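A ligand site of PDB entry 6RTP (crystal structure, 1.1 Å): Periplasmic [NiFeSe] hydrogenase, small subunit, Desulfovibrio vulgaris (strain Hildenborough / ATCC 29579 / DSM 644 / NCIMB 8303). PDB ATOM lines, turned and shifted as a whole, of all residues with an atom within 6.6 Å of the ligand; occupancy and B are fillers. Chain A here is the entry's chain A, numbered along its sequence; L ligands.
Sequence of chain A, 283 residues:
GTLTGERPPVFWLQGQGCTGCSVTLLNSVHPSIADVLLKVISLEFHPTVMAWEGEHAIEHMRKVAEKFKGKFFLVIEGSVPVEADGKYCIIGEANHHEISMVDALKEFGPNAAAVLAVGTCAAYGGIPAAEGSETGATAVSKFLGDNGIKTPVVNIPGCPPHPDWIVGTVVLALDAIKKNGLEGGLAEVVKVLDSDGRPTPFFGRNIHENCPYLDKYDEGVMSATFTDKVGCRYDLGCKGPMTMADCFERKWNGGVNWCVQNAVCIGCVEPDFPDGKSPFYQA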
ATOM      1  N   ILE A 207      -9.132  23.057  11.897  1.00  0.00           N
ATOM      2  CA  ILE A 207      -8.344  22.323  12.888  1.00  0.00           C
ATOM      3  C   ILE A 207      -7.032  23.044  13.187  1.00  0.00           C
ATOM      4  O   ILE A 207      -6.693  23.349  14.340  1.00  0.00           O
ATOM      5  CB  ILE A 207      -8.103  20.872  12.417  1.00  0.00           C
ATOM      6  CG1 ILE A 207      -9.414  20.076  12.315  1.00  0.00           C
ATOM      7  CG2 ILE A 207      -7.111  20.174  13.348  1.00  0.00           C
ATOM      8  CD1 ILE A 207      -9.952  19.528  13.628  1.00  0.00           C
ATOM      9  N   HIS A 208      -6.240  23.275  12.140  1.00  0.00           N
ATOM     10  CA  HIS A 208      -4.872  23.782  12.298  1.00  0.00           C
ATOM     11  C   HIS A 208      -4.839  25.128  12.998  1.00  0.00           C
ATOM     12  O   HIS A 208      -3.992  25.356  13.870  1.00  0.00           O
ATOM     13  CB  HIS A 208      -4.269  23.839  10.894  1.00  0.00           C
ATOM     14  CG  HIS A 208      -2.937  24.488  10.812  1.00  0.00           C
ATOM     15  ND1 HIS A 208      -1.756  23.836  11.104  1.00  0.00           N
ATOM     16  CD2 HIS A 208      -2.587  25.731  10.390  1.00  0.00           C
ATOM     17  CE1 HIS A 208      -0.741  24.650  10.888  1.00  0.00           C
ATOM     18  NE2 HIS A 208      -1.221  25.816  10.457  1.00  0.00           N
ATOM     19  N   GLU A 209      -5.726  26.050  12.610  1.00  0.00           N
ATOM     20  CA  GLU A 209      -5.673  27.382  13.216  1.00  0.00           C
ATOM     21  C   GLU A 209      -6.038  27.362  14.683  1.00  0.00           C
ATOM     22  O   GLU A 209      -5.782  28.362  15.358  1.00  0.00           O
ATOM     23  CB  GLU A 209      -6.550  28.377  12.447  1.00  0.00           C
ATOM     24  CG  GLU A 209      -6.138  28.558  10.985  1.00  0.00           C
ATOM     25  CD  GLU A 209      -4.702  29.062  10.803  1.00  0.00           C
ATOM     26  OE1 GLU A 209      -4.163  29.748  11.695  1.00  0.00           O
ATOM     27  OE2 GLU A 209      -4.098  28.774   9.743  1.00  0.00           O
ATOM     28  N   CYS A 211      -5.070  24.549  16.616  1.00  0.00           N
ATOM     29  CA  CYS A 211      -4.353  23.367  17.093  1.00  0.00           C
ATOM     30  C   CYS A 211      -3.360  23.737  18.200  1.00  0.00           C
ATOM     31  O   CYS A 211      -2.651  24.748  18.091  1.00  0.00           O
ATOM     32  CB  CYS A 211      -3.575  22.729  15.955  1.00  0.00           C
ATOM     33  SG  CYS A 211      -2.674  21.252  16.458  1.00  0.00           S
ATOM     34  N   PRO A 212      -3.250  22.912  19.247  1.00  0.00           N
ATOM     35  CA  PRO A 212      -2.286  23.209  20.302  1.00  0.00           C
ATOM     36  C   PRO A 212      -0.829  23.145  19.868  1.00  0.00           C
ATOM     37  O   PRO A 212       0.033  23.631  20.604  1.00  0.00           O
ATOM     38  CB  PRO A 212      -2.596  22.161  21.385  1.00  0.00           C
ATOM     39  CG  PRO A 212      -3.274  21.099  20.715  1.00  0.00           C
ATOM     40  CD  PRO A 212      -4.057  21.728  19.572  1.00  0.00           C
ATOM     41  N   TYR A 213      -0.523  22.563  18.703  1.00  0.00           N
ATOM     42  CA  TYR A 213       0.848  22.469  18.207  1.00  0.00           C
ATOM     43  C   TYR A 213       1.137  23.526  17.164  1.00  0.00           C
ATOM     44  O   TYR A 213       2.210  23.489  16.552  1.00  0.00           O
ATOM     45  CB  TYR A 213       1.137  21.045  17.688  1.00  0.00           C
ATOM     46  CG  TYR A 213       0.663  20.005  18.671  1.00  0.00           C
ATOM     47  CD1 TYR A 213       1.254  19.878  19.913  1.00  0.00           C
ATOM     48  CD2 TYR A 213      -0.437  19.211  18.386  1.00  0.00           C
ATOM     49  CE1 TYR A 213       0.773  18.947  20.824  1.00  0.00           C
ATOM     50  CE2 TYR A 213      -0.913  18.301  19.294  1.00  0.00           C
ATOM     51  CZ  TYR A 213      -0.310  18.168  20.501  1.00  0.00           C
ATOM     52  OH  TYR A 213      -0.840  17.238  21.374  1.00  0.00           O
ATOM     53  N   LEU A 214       0.244  24.505  17.002  1.00  0.00           N
ATOM     54  CA  LEU A 214       0.416  25.539  15.995  1.00  0.00           C
ATOM     55  C   LEU A 214       1.711  26.332  16.204  1.00  0.00           C
ATOM     56  O   LEU A 214       2.379  26.692  15.233  1.00  0.00           O
ATOM     57  CB  LEU A 214      -0.787  26.465  16.000  1.00  0.00           C
ATOM     58  CG  LEU A 214      -0.824  27.562  14.933  1.00  0.00           C
ATOM     59  CD1 LEU A 214      -0.740  26.994  13.524  1.00  0.00           C
ATOM     60  CD2 LEU A 214      -2.055  28.431  15.084  1.00  0.00           C
ATOM     61  N   ASP A 215       2.088  26.608  17.461  1.00  0.00           N
ATOM     62  CA  ASP A 215       3.345  27.302  17.708  1.00  0.00           C
ATOM     63  C   ASP A 215       4.518  26.516  17.142  1.00  0.00           C
ATOM     64  O   ASP A 215       5.457  27.078  16.567  1.00  0.00           O
ATOM     65  CB  ASP A 215       3.551  27.523  19.211  1.00  0.00           C
ATOM     66  CG  ASP A 215       2.649  28.591  19.789  1.00  0.00           C
ATOM     67  OD1 ASP A 215       1.922  29.267  19.023  1.00  0.00           O
ATOM     68  OD2 ASP A 215       2.648  28.744  21.029  1.00  0.00           O
ATOM     69  N   LYS A 216       4.503  25.193  17.307  1.00  0.00           N
ATOM     70  CA  LYS A 216       5.589  24.361  16.796  1.00  0.00           C
ATOM     71  C   LYS A 216       5.611  24.381  15.278  1.00  0.00           C
ATOM     72  O   LYS A 216       6.678  24.451  14.668  1.00  0.00           O
ATOM     73  CB  LYS A 216       5.462  22.932  17.312  1.00  0.00           C
ATOM     74  CG  LYS A 216       5.492  22.841  18.826  1.00  0.00           C
ATOM     75  CD  LYS A 216       6.770  23.383  19.405  1.00  0.00           C
ATOM     76  CE  LYS A 216       6.754  23.249  20.905  1.00  0.00           C
ATOM     77  NZ  LYS A 216       8.051  23.659  21.436  1.00  0.00           N
ATOM     78  N   TYR A 217       4.438  24.317  14.644  1.00  0.00           N
ATOM     79  CA  TYR A 217       4.372  24.453  13.187  1.00  0.00           C
ATOM     80  C   TYR A 217       5.041  25.744  12.742  1.00  0.00           C
ATOM     81  O   TYR A 217       5.896  25.744  11.846  1.00  0.00           O
ATOM     82  CB  TYR A 217       2.915  24.453  12.748  1.00  0.00           C
ATOM     83  CG  TYR A 217       2.720  24.705  11.274  1.00  0.00           C
ATOM     84  CD1 TYR A 217       2.694  23.660  10.353  1.00  0.00           C
ATOM     85  CD2 TYR A 217       2.520  26.002  10.800  1.00  0.00           C
ATOM     86  CE1 TYR A 217       2.504  23.911   9.014  1.00  0.00           C
ATOM     87  CE2 TYR A 217       2.334  26.249   9.470  1.00  0.00           C
ATOM     88  CZ  TYR A 217       2.324  25.199   8.575  1.00  0.00           C
ATOM     89  OH  TYR A 217       2.130  25.442   7.234  1.00  0.00           O
ATOM     90  N   ASP A 218       4.654  26.862  13.349  1.00  0.00           N
ATOM     91  CA  ASP A 218       5.189  28.161  12.940  1.00  0.00           C
ATOM     92  C   ASP A 218       6.687  28.244  13.204  1.00  0.00           C
ATOM     93  O   ASP A 218       7.398  28.953  12.488  1.00  0.00           O
ATOM     94  CB  ASP A 218       4.447  29.296  13.639  1.00  0.00           C
ATOM     95  CG  ASP A 218       3.038  29.484  13.120  1.00  0.00           C
ATOM     96  OD1 ASP A 218       2.800  29.201  11.927  1.00  0.00           O
ATOM     97  OD2 ASP A 218       2.168  29.934  13.905  1.00  0.00           O
ATOM     98  N   MET A 222       9.182  19.977  13.936  1.00  0.00           N
ATOM     99  CA  MET A 222       8.366  18.893  13.399  1.00  0.00           C
ATOM    100  C   MET A 222       8.816  17.571  13.996  1.00  0.00           C
ATOM    101  O   MET A 222      10.003  17.255  13.960  1.00  0.00           O
ATOM    102  CB  MET A 222       8.562  18.801  11.891  1.00  0.00           C
ATOM    103  CG  MET A 222       8.130  20.044  11.151  1.00  0.00           C
ATOM    104  SD  MET A 222       6.345  20.231  11.306  1.00  0.00           S
ATOM    105  CE  MET A 222       6.146  21.811  10.464  1.00  0.00           C
ATOM    106  N   GLY A 231       6.552  18.005  18.958  1.00  0.00           N
ATOM    107  CA  GLY A 231       6.561  18.696  17.682  1.00  0.00           C
ATOM    108  C   GLY A 231       5.216  18.649  16.969  1.00  0.00           C
ATOM    109  O   GLY A 231       4.297  17.914  17.296  1.00  0.00           O
ATOM    110  N   CYS A 232       5.135  19.508  15.952  1.00  0.00           N
ATOM    111  CA  CYS A 232       4.005  19.473  15.021  1.00  0.00           C
ATOM    112  C   CYS A 232       4.078  18.204  14.173  1.00  0.00           C
ATOM    113  O   CYS A 232       5.171  17.676  13.898  1.00  0.00           O
ATOM    114  CB  CYS A 232       4.038  20.744  14.171  1.00  0.00           C
ATOM    115  SG  CYS A 232       3.019  20.759  12.668  1.00  0.00           S
ATOM    116  N   ARG A 233       2.900  17.724  13.754  1.00  0.00           N
ATOM    117  CA  ARG A 233       2.734  16.492  13.013  1.00  0.00           C
ATOM    118  C   ARG A 233       2.688  16.686  11.490  1.00  0.00           C
ATOM    119  O   ARG A 233       2.428  15.717  10.760  1.00  0.00           O
ATOM    120  CB  ARG A 233       1.441  15.802  13.482  1.00  0.00           C
ATOM    121  CG  ARG A 233       1.495  15.180  14.878  1.00  0.00           C
ATOM    122  CD  ARG A 233       1.575  16.170  16.030  1.00  0.00           C
ATOM    123  NE  ARG A 233       1.064  15.528  17.237  1.00  0.00           N
ATOM    124  CZ  ARG A 233       1.444  15.779  18.491  1.00  0.00           C
ATOM    125  NH1 ARG A 233       2.382  16.666  18.774  1.00  0.00           N
ATOM    126  NH2 ARG A 233       0.870  15.103  19.471  1.00  0.00           N
ATOM    127  N   TYR A 234       2.964  17.891  11.009  1.00  0.00           N
ATOM    128  CA  TYR A 234       2.840  18.185   9.586  1.00  0.00           C
ATOM    129  C   TYR A 234       3.710  17.263   8.717  1.00  0.00           C
ATOM    130  O   TYR A 234       3.233  16.735   7.708  1.00  0.00           O
ATOM    131  CB  TYR A 234       3.203  19.644   9.333  1.00  0.00           C
ATOM    132  CG  TYR A 234       3.072  20.071   7.902  1.00  0.00           C
ATOM    133  CD1 TYR A 234       1.836  20.388   7.368  1.00  0.00           C
ATOM    134  CD2 TYR A 234       4.170  20.162   7.072  1.00  0.00           C
ATOM    135  CE1 TYR A 234       1.705  20.779   6.080  1.00  0.00           C
ATOM    136  CE2 TYR A 234       4.052  20.554   5.766  1.00  0.00           C
ATOM    137  CZ  TYR A 234       2.811  20.861   5.267  1.00  0.00           C
ATOM    138  OH  TYR A 234       2.673  21.262   3.963  1.00  0.00           O
ATOM    139  N   ASP A 235       4.984  17.080   9.068  1.00  0.00           N
ATOM    140  CA  ASP A 235       5.835  16.238   8.230  1.00  0.00           C
ATOM    141  C   ASP A 235       5.409  14.777   8.261  1.00  0.00           C
ATOM    142  O   ASP A 235       5.718  14.042   7.309  1.00  0.00           O
ATOM    143  CB  ASP A 235       7.301  16.315   8.671  1.00  0.00           C
ATOM    144  CG  ASP A 235       7.979  17.615   8.290  1.00  0.00           C
ATOM    145  OD1 ASP A 235       7.381  18.428   7.551  1.00  0.00           O
ATOM    146  OD2 ASP A 235       9.136  17.818   8.735  1.00  0.00           O
ATOM    147  N   CYS A 238       0.026  15.279   8.745  1.00  0.00           N
ATOM    148  CA  CYS A 238      -1.186  15.896   9.284  1.00  0.00           C
ATOM    149  C   CYS A 238      -1.858  16.794   8.253  1.00  0.00           C
ATOM    150  O   CYS A 238      -1.220  17.688   7.683  1.00  0.00           O
ATOM    151  CB  CYS A 238      -0.834  16.698  10.529  1.00  0.00           C
ATOM    152  SG  CYS A 238      -2.300  17.352  11.373  1.00  0.00           S
ATOM    153  N   LYS A 239      -3.164  16.593   8.063  1.00  0.00           N
ATOM    154  CA  LYS A 239      -3.955  17.402   7.130  1.00  0.00           C
ATOM    155  C   LYS A 239      -4.813  18.438   7.843  1.00  0.00           C
ATOM    156  O   LYS A 239      -5.744  18.998   7.243  1.00  0.00           O
ATOM    157  CB  LYS A 239      -4.832  16.515   6.258  1.00  0.00           C
ATOM    158  CG  LYS A 239      -4.046  15.451   5.451  1.00  0.00           C
ATOM    159  CD  LYS A 239      -2.859  16.022   4.689  1.00  0.00           C
ATOM    160  CE  LYS A 239      -2.207  15.029   3.727  1.00  0.00           C
ATOM    161  NZ  LYS A 239      -1.849  13.788   4.393  1.00  0.00           N
ATOM    162  N   GLY A 240      -4.530  18.717   9.124  1.00  0.00           N
ATOM    163  CA  GLY A 240      -5.244  19.755   9.828  1.00  0.00           C
ATOM    164  C   GLY A 240      -5.348  21.070   9.087  1.00  0.00           C
ATOM    165  O   GLY A 240      -6.391  21.732   9.160  1.00  0.00           O
ATOM    166  N   PRO A 241      -4.322  21.498   8.363  1.00  0.00           N
ATOM    167  CA  PRO A 241      -4.443  22.784   7.665  1.00  0.00           C
ATOM    168  C   PRO A 241      -5.604  22.870   6.694  1.00  0.00           C
ATOM    169  O   PRO A 241      -6.137  23.972   6.467  1.00  0.00           O
ATOM    170  CB  PRO A 241      -3.082  22.923   6.968  1.00  0.00           C
ATOM    171  CG  PRO A 241      -2.152  22.193   7.875  1.00  0.00           C
ATOM    172  CD  PRO A 241      -2.930  20.989   8.325  1.00  0.00           C
ATOM    173  N   TRP A 258      -7.593  12.457  20.578  1.00  0.00           N
ATOM    174  CA  TRP A 258      -8.042  12.834  19.244  1.00  0.00           C
ATOM    175  C   TRP A 258      -6.906  12.565  18.287  1.00  0.00           C
ATOM    176  O   TRP A 258      -5.776  12.287  18.682  1.00  0.00           O
ATOM    177  CB  TRP A 258      -8.532  14.280  19.144  1.00  0.00           C
ATOM    178  CG  TRP A 258      -7.526  15.359  19.340  1.00  0.00           C
ATOM    179  CD1 TRP A 258      -6.747  15.579  20.445  1.00  0.00           C
ATOM    180  CD2 TRP A 258      -7.235  16.420  18.425  1.00  0.00           C
ATOM    181  NE1 TRP A 258      -5.973  16.691  20.247  1.00  0.00           N
ATOM    182  CE2 TRP A 258      -6.263  17.245  19.022  1.00  0.00           C
ATOM    183  CE3 TRP A 258      -7.713  16.768  17.152  1.00  0.00           C
ATOM    184  CZ2 TRP A 258      -5.761  18.395  18.405  1.00  0.00           C
ATOM    185  CZ3 TRP A 258      -7.211  17.918  16.535  1.00  0.00           C
ATOM    186  CH2 TRP A 258      -6.243  18.701  17.160  1.00  0.00           C
ATOM    187  N   VAL A 260      -4.966  14.172  16.168  1.00  0.00           N
ATOM    188  CA  VAL A 260      -3.719  14.921  16.086  1.00  0.00           C
ATOM    189  C   VAL A 260      -2.832  14.616  17.287  1.00  0.00           C
ATOM    190  O   VAL A 260      -1.610  14.502  17.148  1.00  0.00           O
ATOM    191  CB  VAL A 260      -3.975  16.430  15.903  1.00  0.00           C
ATOM    192  CG1 VAL A 260      -2.677  17.207  16.013  1.00  0.00           C
ATOM    193  CG2 VAL A 260      -4.643  16.676  14.554  1.00  0.00           C
ATOM    194  N   ALA A 263      -1.777  10.707  16.541  1.00  0.00           N
ATOM    195  CA  ALA A 263      -1.089  10.402  15.301  1.00  0.00           C
ATOM    196  C   ALA A 263      -1.163  11.619  14.387  1.00  0.00           C
ATOM    197  O   ALA A 263      -0.452  12.603  14.641  1.00  0.00           O
ATOM    198  CB  ALA A 263      -1.663   9.139  14.663  1.00  0.00           C
ATOM    199  N   CYS A 265      -4.128  14.005  11.716  1.00  0.00           N
ATOM    200  CA  CYS A 265      -5.436  14.170  11.082  1.00  0.00           C
ATOM    201  C   CYS A 265      -5.323  13.742   9.624  1.00  0.00           C
ATOM    202  O   CYS A 265      -4.347  14.085   8.953  1.00  0.00           O
ATOM    203  CB  CYS A 265      -5.863  15.643  11.194  1.00  0.00           C
ATOM    204  SG  CYS A 265      -7.402  16.085  10.307  1.00  0.00           S
HETATM  205 FE1  LIG L   1      -1.444  19.306  12.279  1.00  0.00          FE
HETATM  206 FE2  LIG L   1      -1.405  22.047  12.037  1.00  0.00          FE
HETATM  207 FE3  LIG L   1       0.777  20.784  13.053  1.00  0.00          FE
HETATM  208 FE4  LIG L   1      -1.571  20.931  14.463  1.00  0.00          FE
HETATM  209  S1  LIG L   1      -0.198  22.665  13.912  1.00  0.00           S
HETATM  210  S2  LIG L   1      -0.203  19.101  14.241  1.00  0.00           S
HETATM  211  S3  LIG L   1      -3.137  20.767  12.770  1.00  0.00           S
HETATM  212  S4  LIG L   1      -0.080  20.534  10.908  1.00  0.00           S
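The backbone NH of Arg 233 lies close to a sulfur (S2) of the ligand, 3.4 Å away.
The side-chain sulfur (SG) of Cys 232 binds an iron atom (FE3) of the ligand, 2.3 Å away.
An iron atom (FE4) of the ligand is bound by the side-chain sulfur (SG) of Cys 211, 2.3 Å away.
ND1 of His 208 binds FE2 of the ligand, 2.0 Å away.
SG of Cys 238 binds FE1 of the ligand, at 2.3 Å.
The backbone NH of Leu 214 sits close to a sulfur (S1) of the ligand.
The guanidinium group (NE) of Arg 233 lies within hydrogen-bond range of the backbone carbonyl oxygen (O) of Val 260, 2.9 Å away.
The backbone NH (N) of Tyr 213 sits close to the side-chain sulfur (SG) of Cys 211, 3.4 Å away.
The backbone NH (N) of Cys 238 sits at hydrogen-bond distance from the backbone carbonyl oxygen (O) of Arg 233 (3.2 Å).
SG of Cys 232 sits close to SD of Met 222, 3.6 Å away.
The side-chain sulfur of Cys 238 lies close to the backbone NH of Gly 240.
O of Gly 240 is in hydrogen-bond range of N of His 208.
The guanidinium group (NH2) of Arg 233 sits at hydrogen-bond distance from the side-chain hydroxyl (OH) of Tyr 213.
The side-chain sulfur (SG) of Cys 232 lies close to the backbone NH (N) of Tyr 234 (3.3 Å).
A sulfur (S1) of the ligand lies close to the backbone carbonyl oxygen (O) of Tyr 213, 3.7 Å away.
Merely in contact with the ligand: Tyr 217, Tyr 234, Gly 240, Pro 241 and Val 260.
Hydrophobic or aromatic side chains that line the ligand: His 208, Tyr 217, Tyr 234, Pro 241 and Val 260.
Within 4 Å of the ligand: His 208, Cys 211, Tyr 213, Leu 214, Tyr 217, Cys 232, Arg 233, Tyr 234, Cys 238, Gly 240, Pro 241 and Val 260.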
